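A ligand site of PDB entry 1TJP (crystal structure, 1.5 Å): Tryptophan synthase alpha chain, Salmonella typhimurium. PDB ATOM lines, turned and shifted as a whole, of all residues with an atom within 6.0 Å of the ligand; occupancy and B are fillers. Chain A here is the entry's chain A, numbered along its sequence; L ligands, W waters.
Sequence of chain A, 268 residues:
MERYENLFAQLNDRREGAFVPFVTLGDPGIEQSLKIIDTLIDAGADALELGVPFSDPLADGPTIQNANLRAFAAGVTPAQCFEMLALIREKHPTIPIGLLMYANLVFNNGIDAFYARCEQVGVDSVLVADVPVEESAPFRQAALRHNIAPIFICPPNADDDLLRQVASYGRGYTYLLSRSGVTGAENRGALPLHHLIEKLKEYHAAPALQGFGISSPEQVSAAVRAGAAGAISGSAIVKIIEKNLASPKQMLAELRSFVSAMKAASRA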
ATOM      1  N   PHE A  22       1.101  20.976  -6.230  1.00  0.00           N
ATOM      2  CA  PHE A  22       2.271  21.038  -7.083  1.00  0.00           C
ATOM      3  C   PHE A  22       1.865  21.454  -8.487  1.00  0.00           C
ATOM      4  O   PHE A  22       0.826  21.011  -8.995  1.00  0.00           O
ATOM      5  CB  PHE A  22       3.007  19.688  -7.171  1.00  0.00           C
ATOM      6  CG  PHE A  22       3.928  19.573  -8.370  1.00  0.00           C
ATOM      7  CD1 PHE A  22       3.419  19.292  -9.636  1.00  0.00           C
ATOM      8  CD2 PHE A  22       5.287  19.799  -8.246  1.00  0.00           C
ATOM      9  CE1 PHE A  22       4.256  19.232 -10.761  1.00  0.00           C
ATOM     10  CE2 PHE A  22       6.138  19.750  -9.355  1.00  0.00           C
ATOM     11  CZ  PHE A  22       5.619  19.476 -10.616  1.00  0.00           C
ATOM     12  N   GLU A  49       4.834  23.213  -4.009  1.00  0.00           N
ATOM     13  CA  GLU A  49       5.930  22.429  -4.606  1.00  0.00           C
ATOM     14  C   GLU A  49       5.898  22.892  -6.084  1.00  0.00           C
ATOM     15  O   GLU A  49       4.825  22.871  -6.751  1.00  0.00           O
ATOM     16  CB  GLU A  49       5.679  20.935  -4.499  1.00  0.00           C
ATOM     17  CG  GLU A  49       6.871  20.156  -4.976  1.00  0.00           C
ATOM     18  CD  GLU A  49       6.571  18.693  -5.253  1.00  0.00           C
ATOM     19  OE1 GLU A  49       5.766  18.101  -4.550  1.00  0.00           O
ATOM     20  OE2 GLU A  49       7.166  18.175  -6.213  1.00  0.00           O
ATOM     21  N   ALA A  59      10.545  10.649 -13.537  1.00  0.00           N
ATOM     22  CA  ALA A  59       9.725  10.172 -12.394  1.00  0.00           C
ATOM     23  C   ALA A  59       8.279  10.612 -12.569  1.00  0.00           C
ATOM     24  O   ALA A  59       7.452  10.446 -11.676  1.00  0.00           O
ATOM     25  CB  ALA A  59      10.265  10.738 -11.044  1.00  0.00           C
ATOM     26  N   ASP A  60       7.963  11.185 -13.739  1.00  0.00           N
ATOM     27  CA  ASP A  60       6.602  11.682 -13.964  1.00  0.00           C
ATOM     28  C   ASP A  60       5.759  10.954 -14.998  1.00  0.00           C
ATOM     29  O   ASP A  60       6.251  10.578 -16.064  1.00  0.00           O
ATOM     30  CB  ASP A  60       6.682  13.165 -14.390  1.00  0.00           C
ATOM     31  CG  ASP A  60       7.052  14.085 -13.226  1.00  0.00           C
ATOM     32  OD1 ASP A  60       6.218  14.137 -12.287  1.00  0.00           O
ATOM     33  OD2 ASP A  60       8.152  14.733 -13.262  1.00  0.00           O
ATOM     34  N   ILE A  64       2.093  15.212 -15.862  1.00  0.00           N
ATOM     35  CA  ILE A  64       3.179  16.163 -15.638  1.00  0.00           C
ATOM     36  C   ILE A  64       4.171  16.186 -16.842  1.00  0.00           C
ATOM     37  O   ILE A  64       4.757  17.220 -17.136  1.00  0.00           O
ATOM     38  CB  ILE A  64       3.803  15.910 -14.244  1.00  0.00           C
ATOM     39  CG1 ILE A  64       2.807  16.440 -13.199  1.00  0.00           C
ATOM     40  CG2 ILE A  64       5.080  16.737 -14.056  1.00  0.00           C
ATOM     41  CD1 ILE A  64       3.108  15.899 -11.786  1.00  0.00           C
ATOM     42  N   LEU A 100      10.874  21.056  -7.290  1.00  0.00           N
ATOM     43  CA  LEU A 100      11.004  19.689  -7.802  1.00  0.00           C
ATOM     44  C   LEU A 100      11.975  19.813  -8.967  1.00  0.00           C
ATOM     45  O   LEU A 100      11.667  20.431  -9.987  1.00  0.00           O
ATOM     46  CB  LEU A 100       9.642  19.120  -8.243  1.00  0.00           C
ATOM     47  CG  LEU A 100       9.617  17.666  -8.731  1.00  0.00           C
ATOM     48  CD1 LEU A 100      10.293  17.499 -10.120  1.00  0.00           C
ATOM     49  CD2 LEU A 100      10.277  16.800  -7.708  1.00  0.00           C
ATOM     50  N   TYR A 102      15.390  17.976 -11.352  1.00  0.00           N
ATOM     51  CA  TYR A 102      16.006  16.778 -11.889  1.00  0.00           C
ATOM     52  C   TYR A 102      17.491  17.133 -11.821  1.00  0.00           C
ATOM     53  O   TYR A 102      17.874  18.289 -12.017  1.00  0.00           O
ATOM     54  CB  TYR A 102      15.519  16.495 -13.312  1.00  0.00           C
ATOM     55  CG  TYR A 102      14.218  15.715 -13.297  1.00  0.00           C
ATOM     56  CD1 TYR A 102      14.214  14.331 -13.111  1.00  0.00           C
ATOM     57  CD2 TYR A 102      12.997  16.373 -13.388  1.00  0.00           C
ATOM     58  CE1 TYR A 102      13.012  13.612 -13.018  1.00  0.00           C
ATOM     59  CE2 TYR A 102      11.791  15.670 -13.290  1.00  0.00           C
ATOM     60  CZ  TYR A 102      11.808  14.298 -13.119  1.00  0.00           C
ATOM     61  OH  TYR A 102      10.620  13.584 -13.043  1.00  0.00           O
ATOM     62  N   LEU A 127      13.781  19.102  -3.812  1.00  0.00           N
ATOM     63  CA  LEU A 127      13.699  17.641  -4.002  1.00  0.00           C
ATOM     64  C   LEU A 127      14.290  17.382  -5.368  1.00  0.00           C
ATOM     65  O   LEU A 127      13.789  17.915  -6.347  1.00  0.00           O
ATOM     66  CB  LEU A 127      12.236  17.177  -3.929  1.00  0.00           C
ATOM     67  CG  LEU A 127      12.060  15.694  -4.291  1.00  0.00           C
ATOM     68  CD1 LEU A 127      13.015  14.758  -3.557  1.00  0.00           C
ATOM     69  CD2 LEU A 127      10.589  15.336  -3.974  1.00  0.00           C
ATOM     70  N   ALA A 129      14.621  14.666  -7.954  1.00  0.00           N
ATOM     71  CA  ALA A 129      13.931  13.398  -8.130  1.00  0.00           C
ATOM     72  C   ALA A 129      14.796  12.192  -8.453  1.00  0.00           C
ATOM     73  O   ALA A 129      14.421  11.071  -8.049  1.00  0.00           O
ATOM     74  CB  ALA A 129      12.826  13.564  -9.191  1.00  0.00           C
ATOM     75  N   ILE A 153      12.951  11.247  -0.560  1.00  0.00           N
ATOM     76  CA  ILE A 153      11.783  10.419  -0.732  1.00  0.00           C
ATOM     77  C   ILE A 153      12.001   9.124   0.049  1.00  0.00           C
ATOM     78  O   ILE A 153      13.049   8.482  -0.040  1.00  0.00           O
ATOM     79  CB  ILE A 153      11.567  10.065  -2.265  1.00  0.00           C
ATOM     80  CG1 ILE A 153      11.001  11.299  -3.013  1.00  0.00           C
ATOM     81  CG2 ILE A 153      10.561   8.897  -2.435  1.00  0.00           C
ATOM     82  CD1 ILE A 153      10.921  11.163  -4.558  1.00  0.00           C
ATOM     83  N   TYR A 175       9.428  13.371   2.235  1.00  0.00           N
ATOM     84  CA  TYR A 175       8.479  13.032   1.182  1.00  0.00           C
ATOM     85  C   TYR A 175       8.130  11.551   1.298  1.00  0.00           C
ATOM     86  O   TYR A 175       8.955  10.687   0.994  1.00  0.00           O
ATOM     87  CB  TYR A 175       9.090  13.319  -0.197  1.00  0.00           C
ATOM     88  CG  TYR A 175       8.073  13.347  -1.315  1.00  0.00           C
ATOM     89  CD1 TYR A 175       7.385  12.191  -1.689  1.00  0.00           C
ATOM     90  CD2 TYR A 175       7.776  14.531  -1.989  1.00  0.00           C
ATOM     91  CE1 TYR A 175       6.413  12.214  -2.697  1.00  0.00           C
ATOM     92  CE2 TYR A 175       6.813  14.571  -2.985  1.00  0.00           C
ATOM     93  CZ  TYR A 175       6.140  13.412  -3.340  1.00  0.00           C
ATOM     94  OH  TYR A 175       5.165  13.443  -4.307  1.00  0.00           O
ATOM     95  N   ARG A 179       3.299   4.995  -3.189  1.00  0.00           N
ATOM     96  CA  ARG A 179       3.436   3.749  -3.966  1.00  0.00           C
ATOM     97  C   ARG A 179       4.625   3.875  -4.900  1.00  0.00           C
ATOM     98  O   ARG A 179       5.242   4.948  -5.042  1.00  0.00           O
ATOM     99  CB  ARG A 179       2.209   3.572  -4.885  1.00  0.00           C
ATOM    100  CG  ARG A 179       1.911   4.863  -5.712  1.00  0.00           C
ATOM    101  CD  ARG A 179       0.939   4.599  -6.856  1.00  0.00           C
ATOM    102  NE  ARG A 179       0.562   5.830  -7.574  1.00  0.00           N
ATOM    103  CZ  ARG A 179       1.326   6.453  -8.480  1.00  0.00           C
ATOM    104  NH1 ARG A 179       2.536   5.967  -8.791  1.00  0.00           N
ATOM    105  NH2 ARG A 179       0.888   7.575  -9.117  1.00  0.00           N
ATOM    106  N   VAL A 182       5.329   6.101 -11.141  1.00  0.00           N
ATOM    107  CA  VAL A 182       5.591   7.539 -11.421  1.00  0.00           C
ATOM    108  C   VAL A 182       4.372   8.380 -11.023  1.00  0.00           C
ATOM    109  O   VAL A 182       3.318   7.826 -10.706  1.00  0.00           O
ATOM    110  CB  VAL A 182       5.933   7.783 -12.936  1.00  0.00           C
ATOM    111  CG1 VAL A 182       7.302   7.068 -13.267  1.00  0.00           C
ATOM    112  CG2 VAL A 182       4.806   7.302 -13.842  1.00  0.00           C
ATOM    113  N   THR A 183       4.521   9.708 -11.045  1.00  0.00           N
ATOM    114  CA  THR A 183       3.407  10.564 -10.625  1.00  0.00           C
ATOM    115  C   THR A 183       2.154  10.309 -11.497  1.00  0.00           C
ATOM    116  O   THR A 183       2.266   9.923 -12.665  1.00  0.00           O
ATOM    117  CB  THR A 183       3.776  12.068 -10.736  1.00  0.00           C
ATOM    118  OG1 THR A 183       4.083  12.405 -12.105  1.00  0.00           O
ATOM    119  CG2 THR A 183       4.971  12.394  -9.859  1.00  0.00           C
ATOM    120  N   GLY A 184       0.984  10.487 -10.888  1.00  0.00           N
ATOM    121  CA  GLY A 184      -0.265  10.353 -11.658  1.00  0.00           C
ATOM    122  C   GLY A 184      -1.496  10.221 -10.786  1.00  0.00           C
ATOM    123  O   GLY A 184      -1.477   9.414  -9.873  1.00  0.00           O
ATOM    124  N   ALA A 185      -2.540  11.001 -11.054  1.00  0.00           N
ATOM    125  CA  ALA A 185      -3.768  10.963 -10.287  1.00  0.00           C
ATOM    126  C   ALA A 185      -4.557   9.678 -10.572  1.00  0.00           C
ATOM    127  O   ALA A 185      -5.345   9.242  -9.734  1.00  0.00           O
ATOM    128  CB  ALA A 185      -4.640  12.202 -10.629  1.00  0.00           C
ATOM    129  N   ASN A 187      -3.630   6.729 -10.457  1.00  0.00           N
ATOM    130  CA  ASN A 187      -3.107   5.554  -9.772  1.00  0.00           C
ATOM    131  C   ASN A 187      -3.003   5.834  -8.265  1.00  0.00           C
ATOM    132  O   ASN A 187      -2.091   6.521  -7.816  1.00  0.00           O
ATOM    133  CB  ASN A 187      -1.743   5.201 -10.351  1.00  0.00           C
ATOM    134  CG  ASN A 187      -1.315   3.809  -9.980  1.00  0.00           C
ATOM    135  OD1 ASN A 187      -1.368   3.419  -8.809  1.00  0.00           O
ATOM    136  ND2 ASN A 187      -0.926   3.010 -10.981  1.00  0.00           N
ATOM    137  N   GLY A 211       2.811  11.847  -0.813  1.00  0.00           N
ATOM    138  CA  GLY A 211       2.629  12.235  -2.211  1.00  0.00           C
ATOM    139  C   GLY A 211       2.621  11.077  -3.180  1.00  0.00           C
ATOM    140  O   GLY A 211       3.251  10.019  -2.902  1.00  0.00           O
ATOM    141  N   PHE A 212       1.991  11.332  -4.343  1.00  0.00           N
ATOM    142  CA  PHE A 212       1.765  10.387  -5.438  1.00  0.00           C
ATOM    143  C   PHE A 212       0.347   9.822  -5.371  1.00  0.00           C
ATOM    144  O   PHE A 212      -0.021   9.152  -4.401  1.00  0.00           O
ATOM    145  CB  PHE A 212       2.769   9.229  -5.430  1.00  0.00           C
ATOM    146  CG  PHE A 212       4.050   9.509  -6.184  1.00  0.00           C
ATOM    147  CD1 PHE A 212       4.759  10.677  -5.970  1.00  0.00           C
ATOM    148  CD2 PHE A 212       4.546   8.581  -7.091  1.00  0.00           C
ATOM    149  CE1 PHE A 212       5.964  10.923  -6.630  1.00  0.00           C
ATOM    150  CE2 PHE A 212       5.747   8.808  -7.772  1.00  0.00           C
ATOM    151  CZ  PHE A 212       6.454   9.987  -7.538  1.00  0.00           C
ATOM    152  N   GLY A 213      -0.438  10.127  -6.402  1.00  0.00           N
ATOM    153  CA  GLY A 213      -1.819   9.602  -6.504  1.00  0.00           C
ATOM    154  C   GLY A 213      -2.857  10.273  -5.615  1.00  0.00           C
ATOM    155  O   GLY A 213      -4.004   9.781  -5.584  1.00  0.00           O
ATOM    156  N   ILE A 214      -2.503  11.323  -4.883  1.00  0.00           N
ATOM    157  CA  ILE A 214      -3.498  11.996  -3.986  1.00  0.00           C
ATOM    158  C   ILE A 214      -4.348  12.947  -4.843  1.00  0.00           C
ATOM    159  O   ILE A 214      -3.849  13.997  -5.335  1.00  0.00           O
ATOM    160  CB  ILE A 214      -2.800  12.842  -2.883  1.00  0.00           C
ATOM    161  CG1 ILE A 214      -1.828  11.981  -2.066  1.00  0.00           C
ATOM    162  CG2 ILE A 214      -3.873  13.510  -1.966  1.00  0.00           C
ATOM    163  CD1 ILE A 214      -2.506  10.926  -1.243  1.00  0.00           C
ATOM    164  N   ILE A 232       0.406  15.990  -0.455  1.00  0.00           N
ATOM    165  CA  ILE A 232       0.749  16.713  -1.668  1.00  0.00           C
ATOM    166  C   ILE A 232      -0.081  16.205  -2.826  1.00  0.00           C
ATOM    167  O   ILE A 232      -0.297  15.025  -2.961  1.00  0.00           O
ATOM    168  CB  ILE A 232       2.242  16.473  -2.020  1.00  0.00           C
ATOM    169  CG1 ILE A 232       3.150  17.038  -0.949  1.00  0.00           C
ATOM    170  CG2 ILE A 232       2.582  17.156  -3.360  1.00  0.00           C
ATOM    171  CD1 ILE A 232       4.578  16.328  -0.933  1.00  0.00           C
ATOM    172  N   SER A 233      -0.565  17.117  -3.678  1.00  0.00           N
ATOM    173  CA  SER A 233      -1.325  16.728  -4.870  1.00  0.00           C
ATOM    174  C   SER A 233      -0.792  17.498  -6.051  1.00  0.00           C
ATOM    175  O   SER A 233      -0.741  18.750  -6.003  1.00  0.00           O
ATOM    176  CB  SER A 233      -2.839  17.058  -4.711  1.00  0.00           C
ATOM    177  OG  SER A 233      -3.572  16.737  -5.893  1.00  0.00           O
ATOM    178  N   GLY A 234      -0.326  16.746  -7.082  1.00  0.00           N
ATOM    179  CA  GLY A 234       0.217  17.430  -8.264  1.00  0.00           C
ATOM    180  C   GLY A 234      -0.599  17.173  -9.506  1.00  0.00           C
ATOM    181  O   GLY A 234      -1.219  18.114 -10.047  1.00  0.00           O
ATOM    182  N   SER A 235      -0.577  15.927  -9.978  1.00  0.00           N
ATOM    183  CA  SER A 235      -1.298  15.566 -11.214  1.00  0.00           C
ATOM    184  C   SER A 235      -2.766  16.010 -11.177  1.00  0.00           C
ATOM    185  O   SER A 235      -3.235  16.500 -12.201  1.00  0.00           O
ATOM    186  CB  SER A 235      -1.191  14.064 -11.456  1.00  0.00           C
ATOM    187  OG  SER A 235       0.146  13.701 -11.789  1.00  0.00           O
ATOM    188  N   ALA A 236      -3.450  15.895 -10.052  1.00  0.00           N
ATOM    189  CA  ALA A 236      -4.887  16.313 -10.007  1.00  0.00           C
ATOM    190  C   ALA A 236      -5.024  17.810 -10.256  1.00  0.00           C
ATOM    191  O   ALA A 236      -5.979  18.264 -10.912  1.00  0.00           O
ATOM    192  CB  ALA A 236      -5.512  15.940  -8.663  1.00  0.00           C
HETATM  193  C1  LIG L   1       8.180  13.857  -9.420  1.00  0.00           C
HETATM  194  C2  LIG L   1       8.830  13.133  -8.339  1.00  0.00           C
HETATM  195  C3  LIG L   1       8.454  13.577  -7.022  1.00  0.00           C
HETATM  196  C4  LIG L   1       7.529  14.618  -6.751  1.00  0.00           C
HETATM  197  C5  LIG L   1       6.951  15.262  -7.852  1.00  0.00           C
HETATM  198  C6  LIG L   1       7.265  14.905  -9.157  1.00  0.00           C
HETATM  199  O1  LIG L   1       6.682  15.568 -10.197  1.00  0.00           O
HETATM  200  N1  LIG L   1       5.984  16.346  -7.619  1.00  0.00           N
HETATM  201  C7  LIG L   1       4.744  16.011  -6.892  1.00  0.00           C
HETATM  202  C8  LIG L   1       3.981  14.794  -7.455  1.00  0.00           C
HETATM  203  C9  LIG L   1       2.741  14.463  -6.673  1.00  0.00           C
HETATM  204  O2  LIG L   1       2.275  13.161  -7.165  1.00  0.00           O
HETATM  205  P1  LIG L   1       0.968  13.186  -8.112  1.00  0.00           P
HETATM  206  O3  LIG L   1      -0.202  13.893  -7.268  1.00  0.00           O
HETATM  207  O4  LIG L   1       1.304  14.021  -9.483  1.00  0.00           O
HETATM  208  O5  LIG L   1       0.731  11.741  -8.342  1.00  0.00           O
HETATM  209  O6  LIG L   1       5.042  15.804  -5.508  1.00  0.00           O
HETATM  210  O7  LIG L   1       3.576  15.271  -8.770  1.00  0.00           O
HETATM  211  O   HOH W   1      -2.713  13.970  -8.054  1.00  0.00           O
HETATM  212  O   HOH W   2      -0.101  13.017  -4.827  1.00  0.00           O
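The side-chain carboxylate of Asp 60 lies within hydrogen-bond range of an oxygen (O1) of the ligand (2.6 Å).
The side-chain carboxylate (OE1) of Glu 49 sits at hydrogen-bond distance from an oxygen (O6) of the ligand (2.6 Å).
The backbone NH of Ser 235 sits at hydrogen-bond distance from an oxygen (O4) of the ligand (2.7 Å).
OG of Ser 235 lies within hydrogen-bond range of O4 of the ligand.
An oxygen (O6) of the ligand lies within hydrogen-bond range of the side-chain hydroxyl (OH) of Tyr 175, 2.7 Å away.
O5 of the ligand is in hydrogen-bond range of N of Gly 213 (2.8 Å).
An oxygen (O5) of the ligand sits at hydrogen-bond distance from the backbone NH (N) of Gly 184.
N of Gly 234 is in hydrogen-bond range of O3 of the ligand, at 2.9 Å.
O2 of the ligand sits close to N of Phe 212, at 3.4 Å.
The side-chain carboxylate (OD1) of Asp 60 lies within hydrogen-bond range of the side-chain hydroxyl (OG1) of Thr 183 (2.8 Å).
OH of Tyr 102 sits at hydrogen-bond distance from OD2 of Asp 60 (2.7 Å).
OG of Ser 235 lies close to N of Gly 184 (3.4 Å).
The guanidinium group (NH2) of Arg 179 lies within hydrogen-bond range of the backbone carbonyl oxygen (O) of Gly 184, 3.1 Å away.
The backbone NH (N) of Thr 183 lies within hydrogen-bond range of the backbone carbonyl oxygen (O) of Ala 59, at 3.1 Å.
O of Ser 233 lies within hydrogen-bond range of N of Phe 22 (2.9 Å).
The side-chain hydroxyl (OG) of Ser 233 lies within hydrogen-bond range of the backbone carbonyl oxygen (O) of Ile 214, 2.8 Å away.
The backbone NH (N) of Ala 59 sits at hydrogen-bond distance from the side-chain hydroxyl (OH) of Tyr 102, 3.0 Å away.
Merely in contact with the ligand: Phe 22, Ala 59, Ile 64, Leu 100, Thr 183, Ile 232 and Ser 233.
Of the 26 residues printed, 15 come within 4 Å of the ligand.
Along chain A the residues within 4 Å of the ligand span positions 22 to 235.
Water W1 lies within hydrogen-bond range of O3 of the ligand (2.6 Å), N of Ala 236 (2.9 Å), O of Ile 214 (2.9 Å) and N of Ser 235 (3.5 Å).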
